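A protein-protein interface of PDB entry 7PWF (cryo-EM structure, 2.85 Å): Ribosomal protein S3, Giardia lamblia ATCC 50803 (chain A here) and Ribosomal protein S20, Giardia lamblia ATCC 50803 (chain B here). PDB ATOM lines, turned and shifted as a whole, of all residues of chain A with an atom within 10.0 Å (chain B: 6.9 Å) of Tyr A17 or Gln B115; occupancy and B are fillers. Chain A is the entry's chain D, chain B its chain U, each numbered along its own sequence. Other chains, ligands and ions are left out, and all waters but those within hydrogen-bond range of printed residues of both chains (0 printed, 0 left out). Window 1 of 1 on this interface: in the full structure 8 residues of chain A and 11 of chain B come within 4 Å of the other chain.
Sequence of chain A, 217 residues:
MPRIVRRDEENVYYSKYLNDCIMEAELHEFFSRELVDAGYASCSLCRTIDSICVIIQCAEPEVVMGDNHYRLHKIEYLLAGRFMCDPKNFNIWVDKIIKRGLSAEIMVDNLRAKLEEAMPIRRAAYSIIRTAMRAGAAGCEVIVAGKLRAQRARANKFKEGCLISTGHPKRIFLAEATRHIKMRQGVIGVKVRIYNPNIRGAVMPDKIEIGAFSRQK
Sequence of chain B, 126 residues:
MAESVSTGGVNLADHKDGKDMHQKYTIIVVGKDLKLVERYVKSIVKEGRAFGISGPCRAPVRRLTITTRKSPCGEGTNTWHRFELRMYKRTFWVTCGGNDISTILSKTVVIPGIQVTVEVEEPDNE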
ATOM      1  N   VAL A  12      18.709 -20.275   8.326  1.00  0.00           N
ATOM      2  CA  VAL A  12      19.332 -21.130   9.322  1.00  0.00           C
ATOM      3  C   VAL A  12      19.685 -22.491   8.706  1.00  0.00           C
ATOM      4  O   VAL A  12      18.870 -23.415   8.660  1.00  0.00           O
ATOM      5  CB  VAL A  12      18.422 -21.278  10.571  1.00  0.00           C
ATOM      6  CG1 VAL A  12      18.868 -22.435  11.453  1.00  0.00           C
ATOM      7  CG2 VAL A  12      18.404 -19.984  11.376  1.00  0.00           C
ATOM      8  N   TYR A  13      20.909 -22.579   8.186  1.00  0.00           N
ATOM      9  CA  TYR A  13      21.515 -23.838   7.777  1.00  0.00           C
ATOM     10  C   TYR A  13      22.556 -24.317   8.775  1.00  0.00           C
ATOM     11  O   TYR A  13      23.078 -25.426   8.624  1.00  0.00           O
ATOM     12  CB  TYR A  13      22.177 -23.695   6.400  1.00  0.00           C
ATOM     13  CG  TYR A  13      21.219 -23.684   5.234  1.00  0.00           C
ATOM     14  CD1 TYR A  13      20.115 -22.842   5.220  1.00  0.00           C
ATOM     15  CD2 TYR A  13      21.419 -24.513   4.143  1.00  0.00           C
ATOM     16  CE1 TYR A  13      19.240 -22.827   4.151  1.00  0.00           C
ATOM     17  CE2 TYR A  13      20.551 -24.506   3.070  1.00  0.00           C
ATOM     18  CZ  TYR A  13      19.461 -23.664   3.080  1.00  0.00           C
ATOM     19  OH  TYR A  13      18.590 -23.652   2.011  1.00  0.00           O
ATOM     20  N   TYR A  14      22.862 -23.498   9.781  1.00  0.00           N
ATOM     21  CA  TYR A  14      23.908 -23.755  10.754  1.00  0.00           C
ATOM     22  C   TYR A  14      23.439 -24.591  11.935  1.00  0.00           C
ATOM     23  O   TYR A  14      24.276 -25.150  12.658  1.00  0.00           O
ATOM     24  CB  TYR A  14      24.444 -22.425  11.277  1.00  0.00           C
ATOM     25  CG  TYR A  14      24.740 -21.392  10.215  1.00  0.00           C
ATOM     26  CD1 TYR A  14      25.913 -21.433   9.481  1.00  0.00           C
ATOM     27  CD2 TYR A  14      23.831 -20.392   9.932  1.00  0.00           C
ATOM     28  CE1 TYR A  14      26.188 -20.484   8.526  1.00  0.00           C
ATOM     29  CE2 TYR A  14      24.094 -19.444   8.977  1.00  0.00           C
ATOM     30  CZ  TYR A  14      25.276 -19.498   8.275  1.00  0.00           C
ATOM     31  OH  TYR A  14      25.543 -18.552   7.323  1.00  0.00           O
ATOM     32  N   SER A  15      22.126 -24.678  12.158  1.00  0.00           N
ATOM     33  CA  SER A  15      21.596 -25.503  13.235  1.00  0.00           C
ATOM     34  C   SER A  15      21.745 -26.987  12.951  1.00  0.00           C
ATOM     35  O   SER A  15      21.472 -27.802  13.837  1.00  0.00           O
ATOM     36  CB  SER A  15      20.128 -25.164  13.476  1.00  0.00           C
ATOM     37  OG  SER A  15      19.304 -25.721  12.469  1.00  0.00           O
ATOM     38  N   LYS A  16      22.146 -27.350  11.735  1.00  0.00           N
ATOM     39  CA  LYS A  16      22.526 -28.705  11.368  1.00  0.00           C
ATOM     40  C   LYS A  16      23.988 -28.957  11.717  1.00  0.00           C
ATOM     41  O   LYS A  16      24.330 -29.972  12.338  1.00  0.00           O
ATOM     42  CB  LYS A  16      22.285 -28.909   9.866  1.00  0.00           C
ATOM     43  CG  LYS A  16      21.837 -30.296   9.450  1.00  0.00           C
ATOM     44  CD  LYS A  16      20.394 -30.567   9.856  1.00  0.00           C
ATOM     45  CE  LYS A  16      19.802 -31.725   9.060  1.00  0.00           C
ATOM     46  NZ  LYS A  16      20.353 -33.042   9.480  1.00  0.00           N
ATOM     47  N   TYR A  17      24.854 -28.014  11.343  1.00  0.00           N
ATOM     48  CA  TYR A  17      26.277 -28.180  11.591  1.00  0.00           C
ATOM     49  C   TYR A  17      26.585 -28.144  13.080  1.00  0.00           C
ATOM     50  O   TYR A  17      27.498 -28.839  13.536  1.00  0.00           O
ATOM     51  CB  TYR A  17      27.074 -27.103  10.858  1.00  0.00           C
ATOM     52  CG  TYR A  17      28.549 -27.403  10.793  1.00  0.00           C
ATOM     53  CD1 TYR A  17      29.003 -28.639  10.350  1.00  0.00           C
ATOM     54  CD2 TYR A  17      29.488 -26.469  11.192  1.00  0.00           C
ATOM     55  CE1 TYR A  17      30.347 -28.925  10.294  1.00  0.00           C
ATOM     56  CE2 TYR A  17      30.830 -26.748  11.146  1.00  0.00           C
ATOM     57  CZ  TYR A  17      31.255 -27.975  10.697  1.00  0.00           C
ATOM     58  OH  TYR A  17      32.599 -28.255  10.647  1.00  0.00           O
ATOM     59  N   LEU A  18      25.833 -27.358  13.857  1.00  0.00           N
ATOM     60  CA  LEU A  18      26.075 -27.334  15.296  1.00  0.00           C
ATOM     61  C   LEU A  18      25.754 -28.680  15.935  1.00  0.00           C
ATOM     62  O   LEU A  18      26.493 -29.154  16.807  1.00  0.00           O
ATOM     63  CB  LEU A  18      25.270 -26.213  15.951  1.00  0.00           C
ATOM     64  CG  LEU A  18      25.453 -26.045  17.461  1.00  0.00           C
ATOM     65  CD1 LEU A  18      26.805 -25.439  17.776  1.00  0.00           C
ATOM     66  CD2 LEU A  18      24.355 -25.178  18.036  1.00  0.00           C
ATOM     67  N   ASN A  19      24.664 -29.321  15.506  1.00  0.00           N
ATOM     68  CA  ASN A  19      24.321 -30.624  16.064  1.00  0.00           C
ATOM     69  C   ASN A  19      25.304 -31.699  15.627  1.00  0.00           C
ATOM     70  O   ASN A  19      25.621 -32.595  16.415  1.00  0.00           O
ATOM     71  CB  ASN A  19      22.897 -31.006  15.676  1.00  0.00           C
ATOM     72  CG  ASN A  19      21.867 -30.448  16.636  1.00  0.00           C
ATOM     73  OD1 ASN A  19      21.148 -29.510  16.308  1.00  0.00           O
ATOM     74  ND2 ASN A  19      21.794 -31.023  17.827  1.00  0.00           N
ATOM     75  N   ASP A  20      25.811 -31.626  14.393  1.00  0.00           N
ATOM     76  CA  ASP A  20      26.923 -32.508  14.033  1.00  0.00           C
ATOM     77  C   ASP A  20      28.135 -32.267  14.927  1.00  0.00           C
ATOM     78  O   ASP A  20      28.813 -33.219  15.336  1.00  0.00           O
ATOM     79  CB  ASP A  20      27.307 -32.352  12.558  1.00  0.00           C
ATOM     80  CG  ASP A  20      26.236 -32.864  11.605  1.00  0.00           C
ATOM     81  OD1 ASP A  20      25.222 -32.180  11.373  1.00  0.00           O
ATOM     82  OD2 ASP A  20      26.418 -33.974  11.072  1.00  0.00           O
ATOM     83  N   CYS A  21      28.423 -31.002  15.239  1.00  0.00           N
ATOM     84  CA  CYS A  21      29.568 -30.683  16.086  1.00  0.00           C
ATOM     85  C   CYS A  21      29.416 -31.280  17.481  1.00  0.00           C
ATOM     86  O   CYS A  21      30.388 -31.774  18.062  1.00  0.00           O
ATOM     87  CB  CYS A  21      29.742 -29.167  16.172  1.00  0.00           C
ATOM     88  SG  CYS A  21      30.699 -28.441  14.834  1.00  0.00           S
ATOM     89  N   ILE A  22      28.211 -31.224  18.042  1.00  0.00           N
ATOM     90  CA  ILE A  22      27.980 -31.778  19.376  1.00  0.00           C
ATOM     91  C   ILE A  22      27.994 -33.308  19.351  1.00  0.00           C
ATOM     92  O   ILE A  22      28.510 -33.960  20.274  1.00  0.00           O
ATOM     93  CB  ILE A  22      26.663 -31.225  19.953  1.00  0.00           C
ATOM     94  CG1 ILE A  22      26.749 -29.708  20.104  1.00  0.00           C
ATOM     95  CG2 ILE A  22      26.364 -31.846  21.295  1.00  0.00           C
ATOM     96  CD1 ILE A  22      25.460 -28.993  19.826  1.00  0.00           C
ATOM     97  N   MET A  23      27.433 -33.906  18.297  1.00  0.00           N
ATOM     98  CA  MET A  23      27.433 -35.358  18.172  1.00  0.00           C
ATOM     99  C   MET A  23      28.848 -35.909  18.023  1.00  0.00           C
ATOM    100  O   MET A  23      29.141 -37.005  18.512  1.00  0.00           O
ATOM    101  CB  MET A  23      26.557 -35.759  16.984  1.00  0.00           C
ATOM    102  CG  MET A  23      26.611 -37.221  16.588  1.00  0.00           C
ATOM    103  SD  MET A  23      25.908 -37.487  14.944  1.00  0.00           S
ATOM    104  CE  MET A  23      26.682 -39.029  14.483  1.00  0.00           C
ATOM    105  N   GLU A  24      29.735 -35.163  17.361  1.00  0.00           N
ATOM    106  CA  GLU A  24      31.129 -35.577  17.275  1.00  0.00           C
ATOM    107  C   GLU A  24      31.765 -35.690  18.657  1.00  0.00           C
ATOM    108  O   GLU A  24      32.539 -36.622  18.912  1.00  0.00           O
ATOM    109  CB  GLU A  24      31.904 -34.593  16.397  1.00  0.00           C
ATOM    110  CG  GLU A  24      33.190 -35.133  15.805  1.00  0.00           C
ATOM    111  CD  GLU A  24      33.731 -34.260  14.682  1.00  0.00           C
ATOM    112  OE1 GLU A  24      34.961 -34.062  14.611  1.00  0.00           O
ATOM    113  OE2 GLU A  24      32.925 -33.760  13.869  1.00  0.00           O
ATOM    114  N   ALA A  25      31.432 -34.773  19.569  1.00  0.00           N
ATOM    115  CA  ALA A  25      31.983 -34.831  20.921  1.00  0.00           C
ATOM    116  C   ALA A  25      31.386 -35.984  21.716  1.00  0.00           C
ATOM    117  O   ALA A  25      32.096 -36.650  22.483  1.00  0.00           O
ATOM    118  CB  ALA A  25      31.749 -33.507  21.641  1.00  0.00           C
ATOM    119  N   LEU A  45      34.291 -36.944  11.917  1.00  0.00           N
ATOM    120  CA  LEU A  45      32.971 -37.180  11.357  1.00  0.00           C
ATOM    121  C   LEU A  45      32.915 -36.681   9.918  1.00  0.00           C
ATOM    122  O   LEU A  45      33.596 -35.719   9.551  1.00  0.00           O
ATOM    123  CB  LEU A  45      31.893 -36.472  12.195  1.00  0.00           C
ATOM    124  CG  LEU A  45      30.505 -37.093  12.289  1.00  0.00           C
ATOM    125  CD1 LEU A  45      30.613 -38.528  12.731  1.00  0.00           C
ATOM    126  CD2 LEU A  45      29.648 -36.305  13.257  1.00  0.00           C
ATOM    127  N   CYS A  46      32.099 -37.346   9.105  1.00  0.00           N
ATOM    128  CA  CYS A  46      31.895 -36.929   7.718  1.00  0.00           C
ATOM    129  C   CYS A  46      30.558 -37.423   7.182  1.00  0.00           C
ATOM    130  O   CYS A  46      29.653 -37.753   7.948  1.00  0.00           O
ATOM    131  CB  CYS A  46      33.029 -37.432   6.827  1.00  0.00           C
ATOM    132  SG  CYS A  46      32.937 -36.859   5.109  1.00  0.00           S
ATOM    133  N   ILE B  28      24.509 -25.224  -1.384  1.00  0.00           N
ATOM    134  CA  ILE B  28      24.921 -24.548  -0.161  1.00  0.00           C
ATOM    135  C   ILE B  28      26.046 -25.357   0.468  1.00  0.00           C
ATOM    136  O   ILE B  28      25.922 -26.577   0.638  1.00  0.00           O
ATOM    137  CB  ILE B  28      23.740 -24.409   0.814  1.00  0.00           C
ATOM    138  CG1 ILE B  28      22.630 -23.554   0.215  1.00  0.00           C
ATOM    139  CG2 ILE B  28      24.200 -23.812   2.127  1.00  0.00           C
ATOM    140  CD1 ILE B  28      23.093 -22.209  -0.211  1.00  0.00           C
ATOM    141  N   VAL B  29      27.145 -24.686   0.812  1.00  0.00           N
ATOM    142  CA  VAL B  29      28.266 -25.323   1.498  1.00  0.00           C
ATOM    143  C   VAL B  29      28.604 -24.518   2.748  1.00  0.00           C
ATOM    144  O   VAL B  29      28.701 -23.288   2.695  1.00  0.00           O
ATOM    145  CB  VAL B  29      29.493 -25.472   0.577  1.00  0.00           C
ATOM    146  CG1 VAL B  29      29.887 -24.148  -0.014  1.00  0.00           C
ATOM    147  CG2 VAL B  29      30.651 -26.052   1.349  1.00  0.00           C
ATOM    148  N   VAL B  30      28.771 -25.214   3.872  1.00  0.00           N
ATOM    149  CA  VAL B  30      28.963 -24.601   5.182  1.00  0.00           C
ATOM    150  C   VAL B  30      30.104 -25.307   5.902  1.00  0.00           C
ATOM    151  O   VAL B  30      30.214 -26.539   5.857  1.00  0.00           O
ATOM    152  CB  VAL B  30      27.662 -24.654   6.014  1.00  0.00           C
ATOM    153  CG1 VAL B  30      27.928 -24.369   7.478  1.00  0.00           C
ATOM    154  CG2 VAL B  30      26.650 -23.670   5.465  1.00  0.00           C
ATOM    155  N   GLY B  31      30.957 -24.519   6.564  1.00  0.00           N
ATOM    156  CA  GLY B  31      32.077 -25.054   7.320  1.00  0.00           C
ATOM    157  C   GLY B  31      32.718 -24.081   8.295  1.00  0.00           C
ATOM    158  O   GLY B  31      32.711 -22.869   8.074  1.00  0.00           O
ATOM    159  N   LYS B  32      33.308 -24.609   9.366  1.00  0.00           N
ATOM    160  CA  LYS B  32      33.832 -23.802  10.460  1.00  0.00           C
ATOM    161  C   LYS B  32      35.333 -23.559  10.389  1.00  0.00           C
ATOM    162  O   LYS B  32      35.872 -22.883  11.269  1.00  0.00           O
ATOM    163  CB  LYS B  32      33.493 -24.455  11.806  1.00  0.00           C
ATOM    164  CG  LYS B  32      34.327 -25.687  12.132  1.00  0.00           C
ATOM    165  CD  LYS B  32      34.460 -25.877  13.638  1.00  0.00           C
ATOM    166  CE  LYS B  32      35.098 -27.207  13.999  1.00  0.00           C
ATOM    167  NZ  LYS B  32      34.104 -28.308  14.110  1.00  0.00           N
ATOM    168  N   ASP B  33      36.029 -24.083   9.381  1.00  0.00           N
ATOM    169  CA  ASP B  33      37.468 -23.872   9.250  1.00  0.00           C
ATOM    170  C   ASP B  33      37.725 -23.294   7.865  1.00  0.00           C
ATOM    171  O   ASP B  33      37.563 -23.991   6.857  1.00  0.00           O
ATOM    172  CB  ASP B  33      38.247 -25.171   9.474  1.00  0.00           C
ATOM    173  CG  ASP B  33      39.761 -24.977   9.427  1.00  0.00           C
ATOM    174  OD1 ASP B  33      40.258 -24.105   8.687  1.00  0.00           O
ATOM    175  OD2 ASP B  33      40.471 -25.715  10.144  1.00  0.00           O
ATOM    176  N   TYR B  40      37.908 -26.542  -0.786  1.00  0.00           N
ATOM    177  CA  TYR B  40      36.759 -27.111  -1.486  1.00  0.00           C
ATOM    178  C   TYR B  40      36.194 -26.123  -2.502  1.00  0.00           C
ATOM    179  O   TYR B  40      35.937 -26.475  -3.661  1.00  0.00           O
ATOM    180  CB  TYR B  40      35.706 -27.510  -0.452  1.00  0.00           C
ATOM    181  CG  TYR B  40      34.464 -28.201  -0.963  1.00  0.00           C
ATOM    182  CD1 TYR B  40      33.519 -27.523  -1.716  1.00  0.00           C
ATOM    183  CD2 TYR B  40      34.214 -29.528  -0.647  1.00  0.00           C
ATOM    184  CE1 TYR B  40      32.378 -28.152  -2.164  1.00  0.00           C
ATOM    185  CE2 TYR B  40      33.074 -30.163  -1.083  1.00  0.00           C
ATOM    186  CZ  TYR B  40      32.158 -29.473  -1.838  1.00  0.00           C
ATOM    187  OH  TYR B  40      31.021 -30.108  -2.279  1.00  0.00           O
ATOM    188  N   LEU B  85      32.824 -19.418  17.856  1.00  0.00           N
ATOM    189  CA  LEU B  85      32.701 -20.368  16.753  1.00  0.00           C
ATOM    190  C   LEU B  85      32.276 -19.607  15.505  1.00  0.00           C
ATOM    191  O   LEU B  85      31.144 -19.125  15.424  1.00  0.00           O
ATOM    192  CB  LEU B  85      31.691 -21.464  17.086  1.00  0.00           C
ATOM    193  CG  LEU B  85      31.609 -22.681  16.165  1.00  0.00           C
ATOM    194  CD1 LEU B  85      32.644 -23.709  16.482  1.00  0.00           C
ATOM    195  CD2 LEU B  85      30.227 -23.293  16.280  1.00  0.00           C
ATOM    196  N   ARG B  86      33.170 -19.505  14.533  1.00  0.00           N
ATOM    197  CA  ARG B  86      32.899 -18.771  13.309  1.00  0.00           C
ATOM    198  C   ARG B  86      32.628 -19.755  12.180  1.00  0.00           C
ATOM    199  O   ARG B  86      33.400 -20.696  11.975  1.00  0.00           O
ATOM    200  CB  ARG B  86      34.072 -17.858  12.959  1.00  0.00           C
ATOM    201  CG  ARG B  86      34.291 -16.738  13.957  1.00  0.00           C
ATOM    202  CD  ARG B  86      35.276 -15.715  13.438  1.00  0.00           C
ATOM    203  NE  ARG B  86      36.631 -16.243  13.369  1.00  0.00           N
ATOM    204  CZ  ARG B  86      37.684 -15.544  12.959  1.00  0.00           C
ATOM    205  NH1 ARG B  86      37.535 -14.281  12.583  1.00  0.00           N
ATOM    206  NH2 ARG B  86      38.884 -16.106  12.921  1.00  0.00           N
ATOM    207  N   MET B  87      31.532 -19.544  11.462  1.00  0.00           N
ATOM    208  CA  MET B  87      31.145 -20.397  10.349  1.00  0.00           C
ATOM    209  C   MET B  87      31.213 -19.622   9.042  1.00  0.00           C
ATOM    210  O   MET B  87      31.230 -18.390   9.019  1.00  0.00           O
ATOM    211  CB  MET B  87      29.735 -20.954  10.542  1.00  0.00           C
ATOM    212  CG  MET B  87      29.644 -22.124  11.498  1.00  0.00           C
ATOM    213  SD  MET B  87      27.990 -22.241  12.205  1.00  0.00           S
ATOM    214  CE  MET B  87      28.050 -23.854  12.959  1.00  0.00           C
ATOM    215  N   ILE B 111      35.887 -34.116   2.029  1.00  0.00           N
ATOM    216  CA  ILE B 111      36.603 -33.625   3.206  1.00  0.00           C
ATOM    217  C   ILE B 111      35.748 -33.867   4.445  1.00  0.00           C
ATOM    218  O   ILE B 111      34.568 -33.491   4.463  1.00  0.00           O
ATOM    219  CB  ILE B 111      36.955 -32.135   3.069  1.00  0.00           C
ATOM    220  CG1 ILE B 111      37.675 -31.859   1.748  1.00  0.00           C
ATOM    221  CG2 ILE B 111      37.852 -31.708   4.200  1.00  0.00           C
ATOM    222  CD1 ILE B 111      38.349 -30.504   1.694  1.00  0.00           C
ATOM    223  N   PRO B 112      36.286 -34.488   5.501  1.00  0.00           N
ATOM    224  CA  PRO B 112      35.505 -34.694   6.730  1.00  0.00           C
ATOM    225  C   PRO B 112      35.451 -33.429   7.572  1.00  0.00           C
ATOM    226  O   PRO B 112      36.440 -33.037   8.200  1.00  0.00           O
ATOM    227  CB  PRO B 112      36.266 -35.824   7.436  1.00  0.00           C
ATOM    228  CG  PRO B 112      37.665 -35.685   6.977  1.00  0.00           C
ATOM    229  CD  PRO B 112      37.657 -35.012   5.621  1.00  0.00           C
ATOM    230  N   GLY B 113      34.284 -32.787   7.594  1.00  0.00           N
ATOM    231  CA  GLY B 113      34.107 -31.561   8.345  1.00  0.00           C
ATOM    232  C   GLY B 113      33.263 -30.527   7.627  1.00  0.00           C
ATOM    233  O   GLY B 113      32.795 -29.562   8.239  1.00  0.00           O
ATOM    234  N   ILE B 114      33.060 -30.722   6.326  1.00  0.00           N
ATOM    235  CA  ILE B 114      32.276 -29.806   5.512  1.00  0.00           C
ATOM    236  C   ILE B 114      30.840 -30.309   5.435  1.00  0.00           C
ATOM    237  O   ILE B 114      30.560 -31.490   5.649  1.00  0.00           O
ATOM    238  CB  ILE B 114      32.890 -29.659   4.110  1.00  0.00           C
ATOM    239  CG1 ILE B 114      32.566 -28.302   3.512  1.00  0.00           C
ATOM    240  CG2 ILE B 114      32.389 -30.756   3.185  1.00  0.00           C
ATOM    241  CD1 ILE B 114      33.438 -27.967   2.333  1.00  0.00           C
ATOM    242  N   GLN B 115      29.912 -29.398   5.134  1.00  0.00           N
ATOM    243  CA  GLN B 115      28.502 -29.748   4.993  1.00  0.00           C
ATOM    244  C   GLN B 115      27.962 -29.163   3.698  1.00  0.00           C
ATOM    245  O   GLN B 115      28.121 -27.968   3.442  1.00  0.00           O
ATOM    246  CB  GLN B 115      27.679 -29.239   6.186  1.00  0.00           C
ATOM    247  CG  GLN B 115      26.210 -29.637   6.137  1.00  0.00           C
ATOM    248  CD  GLN B 115      25.298 -28.578   6.726  1.00  0.00           C
ATOM    249  OE1 GLN B 115      25.758 -27.621   7.345  1.00  0.00           O
ATOM    250  NE2 GLN B 115      23.997 -28.742   6.527  1.00  0.00           N
ATOM    251  N   VAL B 116      27.319 -29.995   2.883  1.00  0.00           N
ATOM    252  CA  VAL B 116      26.785 -29.569   1.593  1.00  0.00           C
ATOM    253  C   VAL B 116      25.338 -30.020   1.481  1.00  0.00           C
ATOM    254  O   VAL B 116      25.024 -31.186   1.743  1.00  0.00           O
ATOM    255  CB  VAL B 116      27.603 -30.129   0.417  1.00  0.00           C
ATOM    256  CG1 VAL B 116      26.938 -29.765  -0.896  1.00  0.00           C
ATOM    257  CG2 VAL B 116      29.026 -29.610   0.455  1.00  0.00           C
ATOM    258  N   THR B 117      24.458 -29.099   1.093  1.00  0.00           N
ATOM    259  CA  THR B 117      23.068 -29.433   0.811  1.00  0.00           C
ATOM    260  C   THR B 117      22.637 -28.781  -0.497  1.00  0.00           C
ATOM    261  O   THR B 117      22.932 -27.606  -0.742  1.00  0.00           O
ATOM    262  CB  THR B 117      22.139 -29.023   1.971  1.00  0.00           C
ATOM    263  OG1 THR B 117      20.788 -29.394   1.668  1.00  0.00           O
ATOM    264  CG2 THR B 117      22.205 -27.527   2.254  1.00  0.00           C
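CG2 of Ile B28 touches CD2 of Tyr A13 (3.5 Å).
Gln B115 touches Tyr A13.
CG2 of Thr B117 touches CE2 of Tyr A13, 3.5 Å away.
Met B87 touches Tyr A14.
CB of Lys A16 touches NE2 of Gln B115 (3.8 Å).
Tyr A17 touches Lys B32 (OH to CG, 3.4 Å).
CE of Met B87 touches CD2 of Tyr A17, at 3.5 Å.
Leu A45 touches Pro B112.
Leu A45 touches Gly B113.
CB of Pro B112 touches CB of Cys A46, at 3.7 Å.
Printed residues of chain A that touch a printed residue of chain B: Tyr A13, Tyr A14, Lys A16, Tyr A17, Cys A21, Leu A45 and Cys A46.
Hydrophobic or aromatic side chains of chain A within 4 Å of the printed part of chain B: Tyr A13, Tyr A14 and Tyr A17.
Of the 17 printed residues of chain B, 8 touch a printed residue of chain A.
Printed residues of chain B that touch a printed residue of chain A: Ile B28, Lys B32, Met B87, Ile B111, Pro B112, Gly B113, Gln B115 and Thr B117.
Hydrophobic or aromatic side chains of chain B within 4 Å of the printed part of chain A: Ile B28, Met B87 and Pro B112.
Along chain B the printed residues that touch a printed residue of chain A span positions 28 to 117.
The backbone carbonyl oxygen (O) of Thr B117 lies within hydrogen-bond range of the backbone NH (N) of Ile B28, 2.9 Å away.
The backbone carbonyl oxygen (O) of Gln B115 sits at hydrogen-bond distance from the backbone NH (N) of Val B30.
O of Lys A16 lies close to OD1 of Asp A20 (2.6 Å).
The backbone carbonyl oxygen of Tyr A17 sits at hydrogen-bond distance from the side-chain sulfur of Cys A21 (3.5 Å).
SG of Cys A21 lies within hydrogen-bond range of NZ of Lys B32.
The side-chain sulfur (SG) of Cys A46 is in hydrogen-bond range of the backbone carbonyl oxygen (O) of Ile B111.
The backbone carbonyl oxygen (O) of Gly B113 lies within hydrogen-bond range of the side-chain hydroxyl (OH) of Tyr A17 (2.7 Å).
Tyr A17 touches just these residues of chain B: Lys B32, Met B87, Gly B113 and Gln B115.
Met A23 touches none of the printed residues of chain B.
Printed residues of chain A within 4 Å of Ile B28: Tyr A13.
No residue of chain A comes within 4 Å of Val B30.
Printed residues of chain A within 4 Å of Lys B32: Tyr A17 and Cys A21.
Leu B85 touches none of the printed residues of chain A.
Of chain A, only Tyr A13 (3.7 Å), Lys A16 (3.8 Å) and Tyr A17 (3.8 Å) come within 4 Å of Gln B115.
No residue of chain A comes within 4 Å of Val B116.
The nearest printed residue of chain B that does not touch Tyr A14 is Val B30 (4.1 Å).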
